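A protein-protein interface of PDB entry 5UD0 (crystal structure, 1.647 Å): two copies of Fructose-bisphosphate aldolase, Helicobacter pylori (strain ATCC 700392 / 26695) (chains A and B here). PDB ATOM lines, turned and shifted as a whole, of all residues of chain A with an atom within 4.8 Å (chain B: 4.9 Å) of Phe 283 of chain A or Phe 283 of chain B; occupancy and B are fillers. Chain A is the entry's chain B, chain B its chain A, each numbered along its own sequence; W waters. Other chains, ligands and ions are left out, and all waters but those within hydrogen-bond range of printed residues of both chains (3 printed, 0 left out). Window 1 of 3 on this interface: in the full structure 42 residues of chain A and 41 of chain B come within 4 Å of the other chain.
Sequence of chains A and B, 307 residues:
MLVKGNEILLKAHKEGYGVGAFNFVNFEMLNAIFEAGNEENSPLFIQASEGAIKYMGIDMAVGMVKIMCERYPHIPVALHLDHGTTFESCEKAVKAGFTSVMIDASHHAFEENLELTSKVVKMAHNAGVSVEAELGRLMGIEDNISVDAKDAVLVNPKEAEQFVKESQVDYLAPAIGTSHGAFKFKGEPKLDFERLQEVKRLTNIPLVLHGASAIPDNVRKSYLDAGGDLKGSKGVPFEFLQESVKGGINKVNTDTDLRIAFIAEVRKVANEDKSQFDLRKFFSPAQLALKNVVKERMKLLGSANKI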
ATOM      1  N   ASN A  26      -0.492  -3.109  21.231  1.00  0.00           N
ATOM      2  CA  ASN A  26       0.072  -4.433  21.048  1.00  0.00           C
ATOM      3  C   ASN A  26      -1.006  -5.482  20.751  1.00  0.00           C
ATOM      4  O   ASN A  26      -2.181  -5.162  20.526  1.00  0.00           O
ATOM      5  CB  ASN A  26       0.886  -4.830  22.278  1.00  0.00           C
ATOM      6  CG  ASN A  26       0.046  -5.029  23.546  1.00  0.00           C
ATOM      7  OD1 ASN A  26      -1.211  -5.112  23.539  1.00  0.00           O
ATOM      8  ND2 ASN A  26       0.759  -5.103  24.681  1.00  0.00           N
ATOM      9  N   GLU A  28      -2.351  -7.973  22.649  1.00  0.00           N
ATOM     10  CA  GLU A  28      -3.404  -8.237  23.621  1.00  0.00           C
ATOM     11  C   GLU A  28      -4.538  -7.214  23.519  1.00  0.00           C
ATOM     12  O   GLU A  28      -5.720  -7.582  23.572  1.00  0.00           O
ATOM     13  CB  GLU A  28      -2.817  -8.245  25.028  1.00  0.00           C
ATOM     14  CG  GLU A  28      -2.162  -9.554  25.389  1.00  0.00           C
ATOM     15  CD  GLU A  28      -0.719  -9.660  24.930  1.00  0.00           C
ATOM     16  OE1 GLU A  28      -0.177  -8.681  24.370  1.00  0.00           O
ATOM     17  OE2 GLU A  28      -0.142 -10.736  25.163  1.00  0.00           O
ATOM     18  N   TYR A  55       6.146   2.386  18.785  1.00  0.00           N
ATOM     19  CA  TYR A  55       6.345   1.255  19.679  1.00  0.00           C
ATOM     20  C   TYR A  55       6.250  -0.062  18.928  1.00  0.00           C
ATOM     21  O   TYR A  55       7.090  -0.948  19.117  1.00  0.00           O
ATOM     22  CB  TYR A  55       5.316   1.336  20.802  1.00  0.00           C
ATOM     23  CG  TYR A  55       5.328   0.208  21.796  1.00  0.00           C
ATOM     24  CD1 TYR A  55       6.240   0.183  22.840  1.00  0.00           C
ATOM     25  CD2 TYR A  55       4.397  -0.829  21.728  1.00  0.00           C
ATOM     26  CE1 TYR A  55       6.240  -0.848  23.776  1.00  0.00           C
ATOM     27  CE2 TYR A  55       4.410  -1.877  22.658  1.00  0.00           C
ATOM     28  CZ  TYR A  55       5.315  -1.867  23.680  1.00  0.00           C
ATOM     29  OH  TYR A  55       5.320  -2.885  24.624  1.00  0.00           O
ATOM     30  N   PHE A 262      -7.193  -2.927  31.729  1.00  0.00           N
ATOM     31  CA  PHE A 262      -6.123  -3.879  31.433  1.00  0.00           C
ATOM     32  C   PHE A 262      -5.090  -3.917  32.554  1.00  0.00           C
ATOM     33  O   PHE A 262      -4.783  -4.980  33.109  1.00  0.00           O
ATOM     34  CB  PHE A 262      -5.468  -3.487  30.109  1.00  0.00           C
ATOM     35  CG  PHE A 262      -4.511  -4.504  29.561  1.00  0.00           C
ATOM     36  CD1 PHE A 262      -4.939  -5.406  28.603  1.00  0.00           C
ATOM     37  CD2 PHE A 262      -3.186  -4.546  29.974  1.00  0.00           C
ATOM     38  CE1 PHE A 262      -4.084  -6.345  28.069  1.00  0.00           C
ATOM     39  CE2 PHE A 262      -2.307  -5.484  29.431  1.00  0.00           C
ATOM     40  CZ  PHE A 262      -2.753  -6.374  28.470  1.00  0.00           C
ATOM     41  N   VAL A 266      -3.408  -6.744  35.460  1.00  0.00           N
ATOM     42  CA  VAL A 266      -1.984  -7.008  35.588  1.00  0.00           C
ATOM     43  C   VAL A 266      -1.552  -6.793  37.034  1.00  0.00           C
ATOM     44  O   VAL A 266      -0.900  -7.656  37.642  1.00  0.00           O
ATOM     45  CB  VAL A 266      -1.196  -6.119  34.605  1.00  0.00           C
ATOM     46  CG1 VAL A 266       0.300  -6.202  34.848  1.00  0.00           C
ATOM     47  CG2 VAL A 266      -1.509  -6.513  33.133  1.00  0.00           C
ATOM     48  N   LEU A 279       3.447 -14.924  31.329  1.00  0.00           N
ATOM     49  CA  LEU A 279       2.819 -13.689  30.846  1.00  0.00           C
ATOM     50  C   LEU A 279       1.336 -13.886  30.568  1.00  0.00           C
ATOM     51  O   LEU A 279       0.537 -12.963  30.782  1.00  0.00           O
ATOM     52  CB  LEU A 279       3.530 -13.162  29.593  1.00  0.00           C
ATOM     53  CG  LEU A 279       4.828 -12.351  29.737  1.00  0.00           C
ATOM     54  CD1 LEU A 279       5.968 -13.166  30.385  1.00  0.00           C
ATOM     55  CD2 LEU A 279       5.220 -11.854  28.347  1.00  0.00           C
ATOM     56  N   ARG A 280       0.941 -15.081  30.117  1.00  0.00           N
ATOM     57  CA  ARG A 280      -0.470 -15.356  29.841  1.00  0.00           C
ATOM     58  C   ARG A 280      -1.346 -15.245  31.088  1.00  0.00           C
ATOM     59  O   ARG A 280      -2.529 -14.880  30.991  1.00  0.00           O
ATOM     60  CB  ARG A 280      -0.604 -16.741  29.215  1.00  0.00           C
ATOM     61  CG  ARG A 280       0.178 -16.909  27.919  1.00  0.00           C
ATOM     62  CD  ARG A 280       0.526 -18.355  27.612  1.00  0.00           C
ATOM     63  NE  ARG A 280       1.609 -18.835  28.476  1.00  0.00           N
ATOM     64  CZ  ARG A 280       2.437 -19.835  28.174  1.00  0.00           C
ATOM     65  NH1 ARG A 280       2.333 -20.482  27.017  1.00  0.00           N
ATOM     66  NH2 ARG A 280       3.382 -20.186  29.035  1.00  0.00           N
ATOM     67  N   LYS A 281      -0.820 -15.612  32.259  1.00  0.00           N
ATOM     68  CA  LYS A 281      -1.604 -15.476  33.484  1.00  0.00           C
ATOM     69  C   LYS A 281      -1.851 -14.018  33.847  1.00  0.00           C
ATOM     70  O   LYS A 281      -2.867 -13.707  34.485  1.00  0.00           O
ATOM     71  CB  LYS A 281      -0.909 -16.208  34.630  1.00  0.00           C
ATOM     72  CG  LYS A 281      -0.901 -17.730  34.485  1.00  0.00           C
ATOM     73  CD  LYS A 281      -2.275 -18.301  34.733  1.00  0.00           C
ATOM     74  CE  LYS A 281      -2.257 -19.815  34.784  1.00  0.00           C
ATOM     75  NZ  LYS A 281      -1.807 -20.398  33.496  1.00  0.00           N
ATOM     76  N   PHE A 282      -0.942 -13.113  33.470  1.00  0.00           N
ATOM     77  CA  PHE A 282      -1.206 -11.682  33.632  1.00  0.00           C
ATOM     78  C   PHE A 282      -2.179 -11.174  32.570  1.00  0.00           C
ATOM     79  O   PHE A 282      -3.109 -10.421  32.876  1.00  0.00           O
ATOM     80  CB  PHE A 282       0.091 -10.854  33.538  1.00  0.00           C
ATOM     81  CG  PHE A 282       1.019 -11.014  34.703  1.00  0.00           C
ATOM     82  CD1 PHE A 282       1.926 -12.055  34.733  1.00  0.00           C
ATOM     83  CD2 PHE A 282       1.004 -10.101  35.753  1.00  0.00           C
ATOM     84  CE1 PHE A 282       2.793 -12.214  35.799  1.00  0.00           C
ATOM     85  CE2 PHE A 282       1.860 -10.250  36.826  1.00  0.00           C
ATOM     86  CZ  PHE A 282       2.762 -11.327  36.841  1.00  0.00           C
ATOM     87  N   PHE A 283      -1.969 -11.559  31.311  1.00  0.00           N
ATOM     88  CA  PHE A 283      -2.610 -10.854  30.206  1.00  0.00           C
ATOM     89  C   PHE A 283      -3.930 -11.476  29.748  1.00  0.00           C
ATOM     90  O   PHE A 283      -4.738 -10.773  29.112  1.00  0.00           O
ATOM     91  CB  PHE A 283      -1.642 -10.735  29.034  1.00  0.00           C
ATOM     92  CG  PHE A 283      -0.370 -10.020  29.384  1.00  0.00           C
ATOM     93  CD1 PHE A 283      -0.361  -9.033  30.374  1.00  0.00           C
ATOM     94  CD2 PHE A 283       0.807 -10.324  28.727  1.00  0.00           C
ATOM     95  CE1 PHE A 283       0.786  -8.385  30.719  1.00  0.00           C
ATOM     96  CE2 PHE A 283       1.977  -9.674  29.059  1.00  0.00           C
ATOM     97  CZ  PHE A 283       1.974  -8.703  30.063  1.00  0.00           C
ATOM     98  N   SER A 284      -4.209 -12.740  30.074  1.00  0.00           N
ATOM     99  CA  SER A 284      -5.538 -13.263  29.764  1.00  0.00           C
ATOM    100  C   SER A 284      -6.608 -12.523  30.543  1.00  0.00           C
ATOM    101  O   SER A 284      -7.558 -12.029  29.922  1.00  0.00           O
ATOM    102  CB  SER A 284      -5.605 -14.773  30.016  1.00  0.00           C
ATOM    103  OG  SER A 284      -4.904 -15.472  28.982  1.00  0.00           O
ATOM    104  N   PRO A 285      -6.524 -12.392  31.866  1.00  0.00           N
ATOM    105  CA  PRO A 285      -7.548 -11.601  32.561  1.00  0.00           C
ATOM    106  C   PRO A 285      -7.561 -10.151  32.126  1.00  0.00           C
ATOM    107  O   PRO A 285      -8.627  -9.554  31.996  1.00  0.00           O
ATOM    108  CB  PRO A 285      -7.173 -11.760  34.039  1.00  0.00           C
ATOM    109  CG  PRO A 285      -5.726 -12.160  34.039  1.00  0.00           C
ATOM    110  CD  PRO A 285      -5.550 -12.986  32.795  1.00  0.00           C
ATOM    111  N   ALA A 286      -6.397  -9.570  31.872  1.00  0.00           N
ATOM    112  CA  ALA A 286      -6.359  -8.186  31.400  1.00  0.00           C
ATOM    113  C   ALA A 286      -7.116  -8.022  30.085  1.00  0.00           C
ATOM    114  O   ALA A 286      -7.865  -7.040  29.896  1.00  0.00           O
ATOM    115  CB  ALA A 286      -4.898  -7.756  31.254  1.00  0.00           C
ATOM    116  N   GLN A 287      -6.906  -8.956  29.147  1.00  0.00           N
ATOM    117  CA  GLN A 287      -7.666  -8.935  27.905  1.00  0.00           C
ATOM    118  C   GLN A 287      -9.159  -9.027  28.184  1.00  0.00           C
ATOM    119  O   GLN A 287      -9.942  -8.314  27.565  1.00  0.00           O
ATOM    120  CB  GLN A 287      -7.275 -10.089  26.971  1.00  0.00           C
ATOM    121  CG  GLN A 287      -5.952  -9.968  26.216  1.00  0.00           C
ATOM    122  CD  GLN A 287      -5.811 -11.090  25.190  1.00  0.00           C
ATOM    123  OE1 GLN A 287      -6.628 -11.221  24.281  1.00  0.00           O
ATOM    124  NE2 GLN A 287      -4.793 -11.919  25.354  1.00  0.00           N
ATOM    125  N   ASN B  26       3.849 -13.353  22.746  1.00  0.00           N
ATOM    126  CA  ASN B  26       3.208 -12.143  22.270  1.00  0.00           C
ATOM    127  C   ASN B  26       4.240 -11.266  21.541  1.00  0.00           C
ATOM    128  O   ASN B  26       5.387 -11.663  21.304  1.00  0.00           O
ATOM    129  CB  ASN B  26       2.533 -11.394  23.430  1.00  0.00           C
ATOM    130  CG  ASN B  26       3.521 -10.754  24.403  1.00  0.00           C
ATOM    131  OD1 ASN B  26       4.740 -10.719  24.181  1.00  0.00           O
ATOM    132  ND2 ASN B  26       2.989 -10.224  25.486  1.00  0.00           N
ATOM    133  N   GLU B  28       5.712  -8.341  22.350  1.00  0.00           N
ATOM    134  CA  GLU B  28       6.839  -7.802  23.105  1.00  0.00           C
ATOM    135  C   GLU B  28       7.977  -8.816  23.221  1.00  0.00           C
ATOM    136  O   GLU B  28       9.152  -8.461  23.039  1.00  0.00           O
ATOM    137  CB  GLU B  28       6.379  -7.350  24.482  1.00  0.00           C
ATOM    138  CG  GLU B  28       5.741  -5.979  24.485  1.00  0.00           C
ATOM    139  CD  GLU B  28       4.237  -5.988  24.193  1.00  0.00           C
ATOM    140  OE1 GLU B  28       3.643  -7.087  24.025  1.00  0.00           O
ATOM    141  OE2 GLU B  28       3.654  -4.885  24.190  1.00  0.00           O
ATOM    142  N   TYR B  55      -2.908 -19.253  22.730  1.00  0.00           N
ATOM    143  CA  TYR B  55      -3.061 -17.900  23.240  1.00  0.00           C
ATOM    144  C   TYR B  55      -3.068 -16.878  22.110  1.00  0.00           C
ATOM    145  O   TYR B  55      -3.925 -15.989  22.073  1.00  0.00           O
ATOM    146  CB  TYR B  55      -1.929 -17.612  24.230  1.00  0.00           C
ATOM    147  CG  TYR B  55      -1.901 -16.219  24.791  1.00  0.00           C
ATOM    148  CD1 TYR B  55      -2.750 -15.847  25.816  1.00  0.00           C
ATOM    149  CD2 TYR B  55      -1.004 -15.281  24.314  1.00  0.00           C
ATOM    150  CE1 TYR B  55      -2.715 -14.593  26.344  1.00  0.00           C
ATOM    151  CE2 TYR B  55      -0.969 -14.005  24.836  1.00  0.00           C
ATOM    152  CZ  TYR B  55      -1.820 -13.669  25.850  1.00  0.00           C
ATOM    153  OH  TYR B  55      -1.790 -12.398  26.373  1.00  0.00           O
ATOM    154  N   PHE B 262      11.361 -10.390  32.061  1.00  0.00           N
ATOM    155  CA  PHE B 262      10.259  -9.557  31.580  1.00  0.00           C
ATOM    156  C   PHE B 262       9.361  -9.125  32.736  1.00  0.00           C
ATOM    157  O   PHE B 262       9.144  -7.929  32.958  1.00  0.00           O
ATOM    158  CB  PHE B 262       9.465 -10.341  30.528  1.00  0.00           C
ATOM    159  CG  PHE B 262       8.463  -9.526  29.771  1.00  0.00           C
ATOM    160  CD1 PHE B 262       8.807  -8.928  28.567  1.00  0.00           C
ATOM    161  CD2 PHE B 262       7.174  -9.377  30.247  1.00  0.00           C
ATOM    162  CE1 PHE B 262       7.891  -8.166  27.853  1.00  0.00           C
ATOM    163  CE2 PHE B 262       6.230  -8.625  29.537  1.00  0.00           C
ATOM    164  CZ  PHE B 262       6.596  -8.029  28.324  1.00  0.00           C
ATOM    165  N   VAL B 266       7.875  -5.536  34.838  1.00  0.00           N
ATOM    166  CA  VAL B 266       6.447  -5.241  34.960  1.00  0.00           C
ATOM    167  C   VAL B 266       6.081  -5.001  36.420  1.00  0.00           C
ATOM    168  O   VAL B 266       5.444  -3.996  36.763  1.00  0.00           O
ATOM    169  CB  VAL B 266       5.623  -6.388  34.359  1.00  0.00           C
ATOM    170  CG1 VAL B 266       4.133  -6.174  34.583  1.00  0.00           C
ATOM    171  CG2 VAL B 266       5.903  -6.506  32.877  1.00  0.00           C
ATOM    172  N   LEU B 279       0.482   1.021  28.973  1.00  0.00           N
ATOM    173  CA  LEU B 279       1.059  -0.311  28.778  1.00  0.00           C
ATOM    174  C   LEU B 279       2.509  -0.236  28.334  1.00  0.00           C
ATOM    175  O   LEU B 279       3.328  -1.084  28.714  1.00  0.00           O
ATOM    176  CB  LEU B 279       0.255  -1.100  27.743  1.00  0.00           C
ATOM    177  CG  LEU B 279      -0.981  -1.872  28.257  1.00  0.00           C
ATOM    178  CD1 LEU B 279      -2.094  -0.921  28.666  1.00  0.00           C
ATOM    179  CD2 LEU B 279      -1.461  -2.860  27.196  1.00  0.00           C
ATOM    180  N   ARG B 280       2.832   0.729  27.465  1.00  0.00           N
ATOM    181  CA  ARG B 280       4.198   0.862  26.963  1.00  0.00           C
ATOM    182  C   ARG B 280       5.185   1.201  28.072  1.00  0.00           C
ATOM    183  O   ARG B 280       6.356   0.804  28.007  1.00  0.00           O
ATOM    184  CB  ARG B 280       4.238   1.918  25.854  1.00  0.00           C
ATOM    185  CG  ARG B 280       3.402   1.548  24.619  1.00  0.00           C
ATOM    186  CD  ARG B 280       3.024   2.766  23.760  1.00  0.00           C
ATOM    187  NE  ARG B 280       2.134   3.648  24.511  1.00  0.00           N
ATOM    188  CZ  ARG B 280       1.479   4.690  24.008  1.00  0.00           C
ATOM    189  NH1 ARG B 280       1.599   5.017  22.726  1.00  0.00           N
ATOM    190  NH2 ARG B 280       0.700   5.412  24.802  1.00  0.00           N
ATOM    191  N   LYS B 281       4.745   1.920  29.105  1.00  0.00           N
ATOM    192  CA  LYS B 281       5.618   2.168  30.247  1.00  0.00           C
ATOM    193  C   LYS B 281       5.928   0.891  31.016  1.00  0.00           C
ATOM    194  O   LYS B 281       6.971   0.802  31.661  1.00  0.00           O
ATOM    195  CB  LYS B 281       4.994   3.188  31.190  1.00  0.00           C
ATOM    196  CG  LYS B 281       4.900   4.584  30.594  1.00  0.00           C
ATOM    197  CD  LYS B 281       6.267   5.228  30.438  1.00  0.00           C
ATOM    198  CE  LYS B 281       6.179   6.608  29.792  1.00  0.00           C
ATOM    199  NZ  LYS B 281       7.516   7.245  29.736  1.00  0.00           N
ATOM    200  N   PHE B 282       5.025  -0.084  31.002  1.00  0.00           N
ATOM    201  CA  PHE B 282       5.340  -1.373  31.605  1.00  0.00           C
ATOM    202  C   PHE B 282       6.229  -2.218  30.706  1.00  0.00           C
ATOM    203  O   PHE B 282       7.171  -2.856  31.186  1.00  0.00           O
ATOM    204  CB  PHE B 282       4.063  -2.146  31.910  1.00  0.00           C
ATOM    205  CG  PHE B 282       3.297  -1.619  33.077  1.00  0.00           C
ATOM    206  CD1 PHE B 282       2.307  -0.656  32.905  1.00  0.00           C
ATOM    207  CD2 PHE B 282       3.545  -2.095  34.345  1.00  0.00           C
ATOM    208  CE1 PHE B 282       1.617  -0.166  33.982  1.00  0.00           C
ATOM    209  CE2 PHE B 282       2.834  -1.616  35.434  1.00  0.00           C
ATOM    210  CZ  PHE B 282       1.890  -0.653  35.255  1.00  0.00           C
ATOM    211  N   PHE B 283       5.953  -2.242  29.406  1.00  0.00           N
ATOM    212  CA  PHE B 283       6.532  -3.276  28.567  1.00  0.00           C
ATOM    213  C   PHE B 283       7.769  -2.840  27.804  1.00  0.00           C
ATOM    214  O   PHE B 283       8.458  -3.699  27.245  1.00  0.00           O
ATOM    215  CB  PHE B 283       5.500  -3.811  27.583  1.00  0.00           C
ATOM    216  CG  PHE B 283       4.263  -4.314  28.245  1.00  0.00           C
ATOM    217  CD1 PHE B 283       4.304  -4.880  29.516  1.00  0.00           C
ATOM    218  CD2 PHE B 283       3.043  -4.175  27.632  1.00  0.00           C
ATOM    219  CE1 PHE B 283       3.147  -5.304  30.142  1.00  0.00           C
ATOM    220  CE2 PHE B 283       1.903  -4.621  28.252  1.00  0.00           C
ATOM    221  CZ  PHE B 283       1.956  -5.184  29.505  1.00  0.00           C
ATOM    222  N   SER B 284       8.082  -1.553  27.751  1.00  0.00           N
ATOM    223  CA  SER B 284       9.362  -1.172  27.161  1.00  0.00           C
ATOM    224  C   SER B 284      10.524  -1.586  28.046  1.00  0.00           C
ATOM    225  O   SER B 284      11.489  -2.163  27.527  1.00  0.00           O
ATOM    226  CB  SER B 284       9.394   0.326  26.866  1.00  0.00           C
ATOM    227  OG  SER B 284       8.614   0.639  25.718  1.00  0.00           O
ATOM    228  N   PRO B 285      10.511  -1.330  29.358  1.00  0.00           N
ATOM    229  CA  PRO B 285      11.597  -1.871  30.181  1.00  0.00           C
ATOM    230  C   PRO B 285      11.599  -3.383  30.207  1.00  0.00           C
ATOM    231  O   PRO B 285      12.676  -3.990  30.226  1.00  0.00           O
ATOM    232  CB  PRO B 285      11.326  -1.260  31.560  1.00  0.00           C
ATOM    233  CG  PRO B 285       9.891  -0.917  31.548  1.00  0.00           C
ATOM    234  CD  PRO B 285       9.588  -0.506  30.148  1.00  0.00           C
ATOM    235  N   ALA B 286      10.417  -4.002  30.185  1.00  0.00           N
ATOM    236  CA  ALA B 286      10.334  -5.458  30.165  1.00  0.00           C
ATOM    237  C   ALA B 286      10.974  -6.028  28.904  1.00  0.00           C
ATOM    238  O   ALA B 286      11.738  -7.000  28.972  1.00  0.00           O
ATOM    239  CB  ALA B 286       8.867  -5.892  30.279  1.00  0.00           C
ATOM    240  N   GLN B 287      10.723  -5.409  27.749  1.00  0.00           N
ATOM    241  CA  GLN B 287      11.391  -5.834  26.517  1.00  0.00           C
ATOM    242  C   GLN B 287      12.911  -5.688  26.616  1.00  0.00           C
ATOM    243  O   GLN B 287      13.652  -6.599  26.245  1.00  0.00           O
ATOM    244  CB  GLN B 287      10.893  -5.033  25.317  1.00  0.00           C
ATOM    245  CG  GLN B 287       9.579  -5.401  24.723  1.00  0.00           C
ATOM    246  CD  GLN B 287       9.334  -4.605  23.456  1.00  0.00           C
ATOM    247  OE1 GLN B 287      10.099  -4.718  22.487  1.00  0.00           O
ATOM    248  NE2 GLN B 287       8.284  -3.766  23.463  1.00  0.00           N
HETATM  249  O   HOH W   1       8.775  -1.846  21.227  1.00  0.00           O
HETATM  250  O   HOH W   2      -5.339 -14.521  24.006  1.00  0.00           O
HETATM  251  O   HOH W   3       1.702  -8.211  22.463  1.00  0.00           O
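The side-chain amide nitrogen of Asn 26 of chain B is in hydrogen-bond range of the side-chain carboxylate of Glu 28 of chain A (3.2 Å).
The side-chain carboxylate (OE2) of Glu 28 of chain B sits at hydrogen-bond distance from the side-chain amide nitrogen (ND2) of Asn 26 of chain A (2.9 Å).
The side-chain carboxylate of Glu 28 of chain B sits at hydrogen-bond distance from the side-chain hydroxyl of Tyr 55 of chain A.
The side-chain hydroxyl (OH) of Tyr 55 of chain B is in hydrogen-bond range of the side-chain carboxylate (OE2) of Glu 28 of chain A, 2.6 Å away.
The side-chain hydroxyl (OH) of Tyr 55 of chain B sits at hydrogen-bond distance from the side-chain amide nitrogen (NE2) of Gln 287 of chain A, 3.2 Å away.
OH of Tyr 55 of chain A sits at hydrogen-bond distance from NE2 of Gln 287 of chain B (3.3 Å).
OD1 of Asn 26 of chain B lies within hydrogen-bond range of N of Glu 28 of chain B (3.2 Å).
The backbone carbonyl oxygen (O) of Arg 280 of chain B is in hydrogen-bond range of the side-chain hydroxyl (OG) of Ser 284 of chain B, at 3.2 Å.
OD1 of Asn 26 of chain A lies within hydrogen-bond range of N of Glu 28 of chain A, at 3.2 Å.
The side-chain hydroxyl of Ser 284 of chain A is in hydrogen-bond range of the backbone carbonyl oxygen of Arg 280 of chain A, at 3.2 Å.
Among the printed residues, merely in contact across the chains: Asn 26 of chain A with Phe 283 of chain B (3.8 Å), Tyr 55 of chain A with Arg 280 of chain B (3.6 Å), Tyr 55 of chain A with Phe 283 of chain B (3.1 Å), Tyr 55 of chain A with Ser 284 of chain B (3.4 Å), Phe 262 of chain A with Leu 279 of chain B (3.5 Å), Val 266 of chain A with Val 266 of chain B (3.8 Å), Leu 279 of chain A with Asn 26 of chain B (3.98 Å), Leu 279 of chain A with Phe 262 of chain B (3.6 Å), Arg 280 of chain A with Tyr 55 of chain B (3.8 Å), Phe 283 of chain A with Asn 26 of chain B (3.8 Å), Phe 283 of chain A with Tyr 55 of chain B (3.1 Å), Phe 283 of chain A with Phe 283 of chain B (3.6 Å) and Ser 284 of chain A with Tyr 55 of chain B (3.5 Å).
Phe 283 of chain A touches three residues of chain B.
Ala 286 of chain A touches none of the printed residues of chain B.
Of the printed residues of chain A, Asn 26 of chain B touches Glu 28, Leu 279 and Phe 283.
Of the printed residues of chain A, Arg 280 of chain B touches Tyr 55 (3.6 Å).
Phe 283 of chain B touches three residues of chain A.
Pro 285 of chain B touches none of the printed residues of chain A.
The nearest printed residue of chain A that does not touch Tyr 55 of chain B is Leu 279 of chain A (5.0 Å).
Hydrophobic or aromatic side chains of chain A that line the printed part of chain B: Tyr 55, Phe 262, Val 266, Leu 279 and Phe 283.
Of the 14 printed residues of chain B, 10 touch a printed residue of chain A.
Hydrophobic or aromatic side chains of chain B that line the printed part of chain A: Tyr 55, Phe 262, Val 266, Leu 279 and Phe 283.
Among the printed residues, 19 pairs touch across the chains.
Among the printed residues, no Asp or Glu carboxylate lies within 4 Å of a Lys or Arg side-chain nitrogen of the other chain.
Glu 28 of chain A touches Tyr 55 of chain B, and with the chains exchanged Tyr 55 of chain A touches Glu 28 of chain B.
Tyr 55 of chain A touches Gln 287 of chain B, and with the chains exchanged Gln 287 of chain A touches Tyr 55 of chain B.
Val 266 of chain A touches its own counterpart, Val 266 of chain B.
Phe 283 of chain A touches its own counterpart, Phe 283 of chain B.
Of the 19 pairs that touch across the chains among the printed residues, 18 have their exchanged pair printed and touching as well.
Water W3 lies within hydrogen-bond range of OE1 of Glu 28 of chain A and OE1 of Glu 28 of chain B.
Water W2 lies within hydrogen-bond range of O of Tyr 55 of chain B (2.8 Å) and NE2 of Gln 287 of chain A (3.0 Å).
Water W1 lies within hydrogen-bond range of O of Tyr 55 of chain A (2.8 Å) and NE2 of Gln 287 of chain B (3.0 Å).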
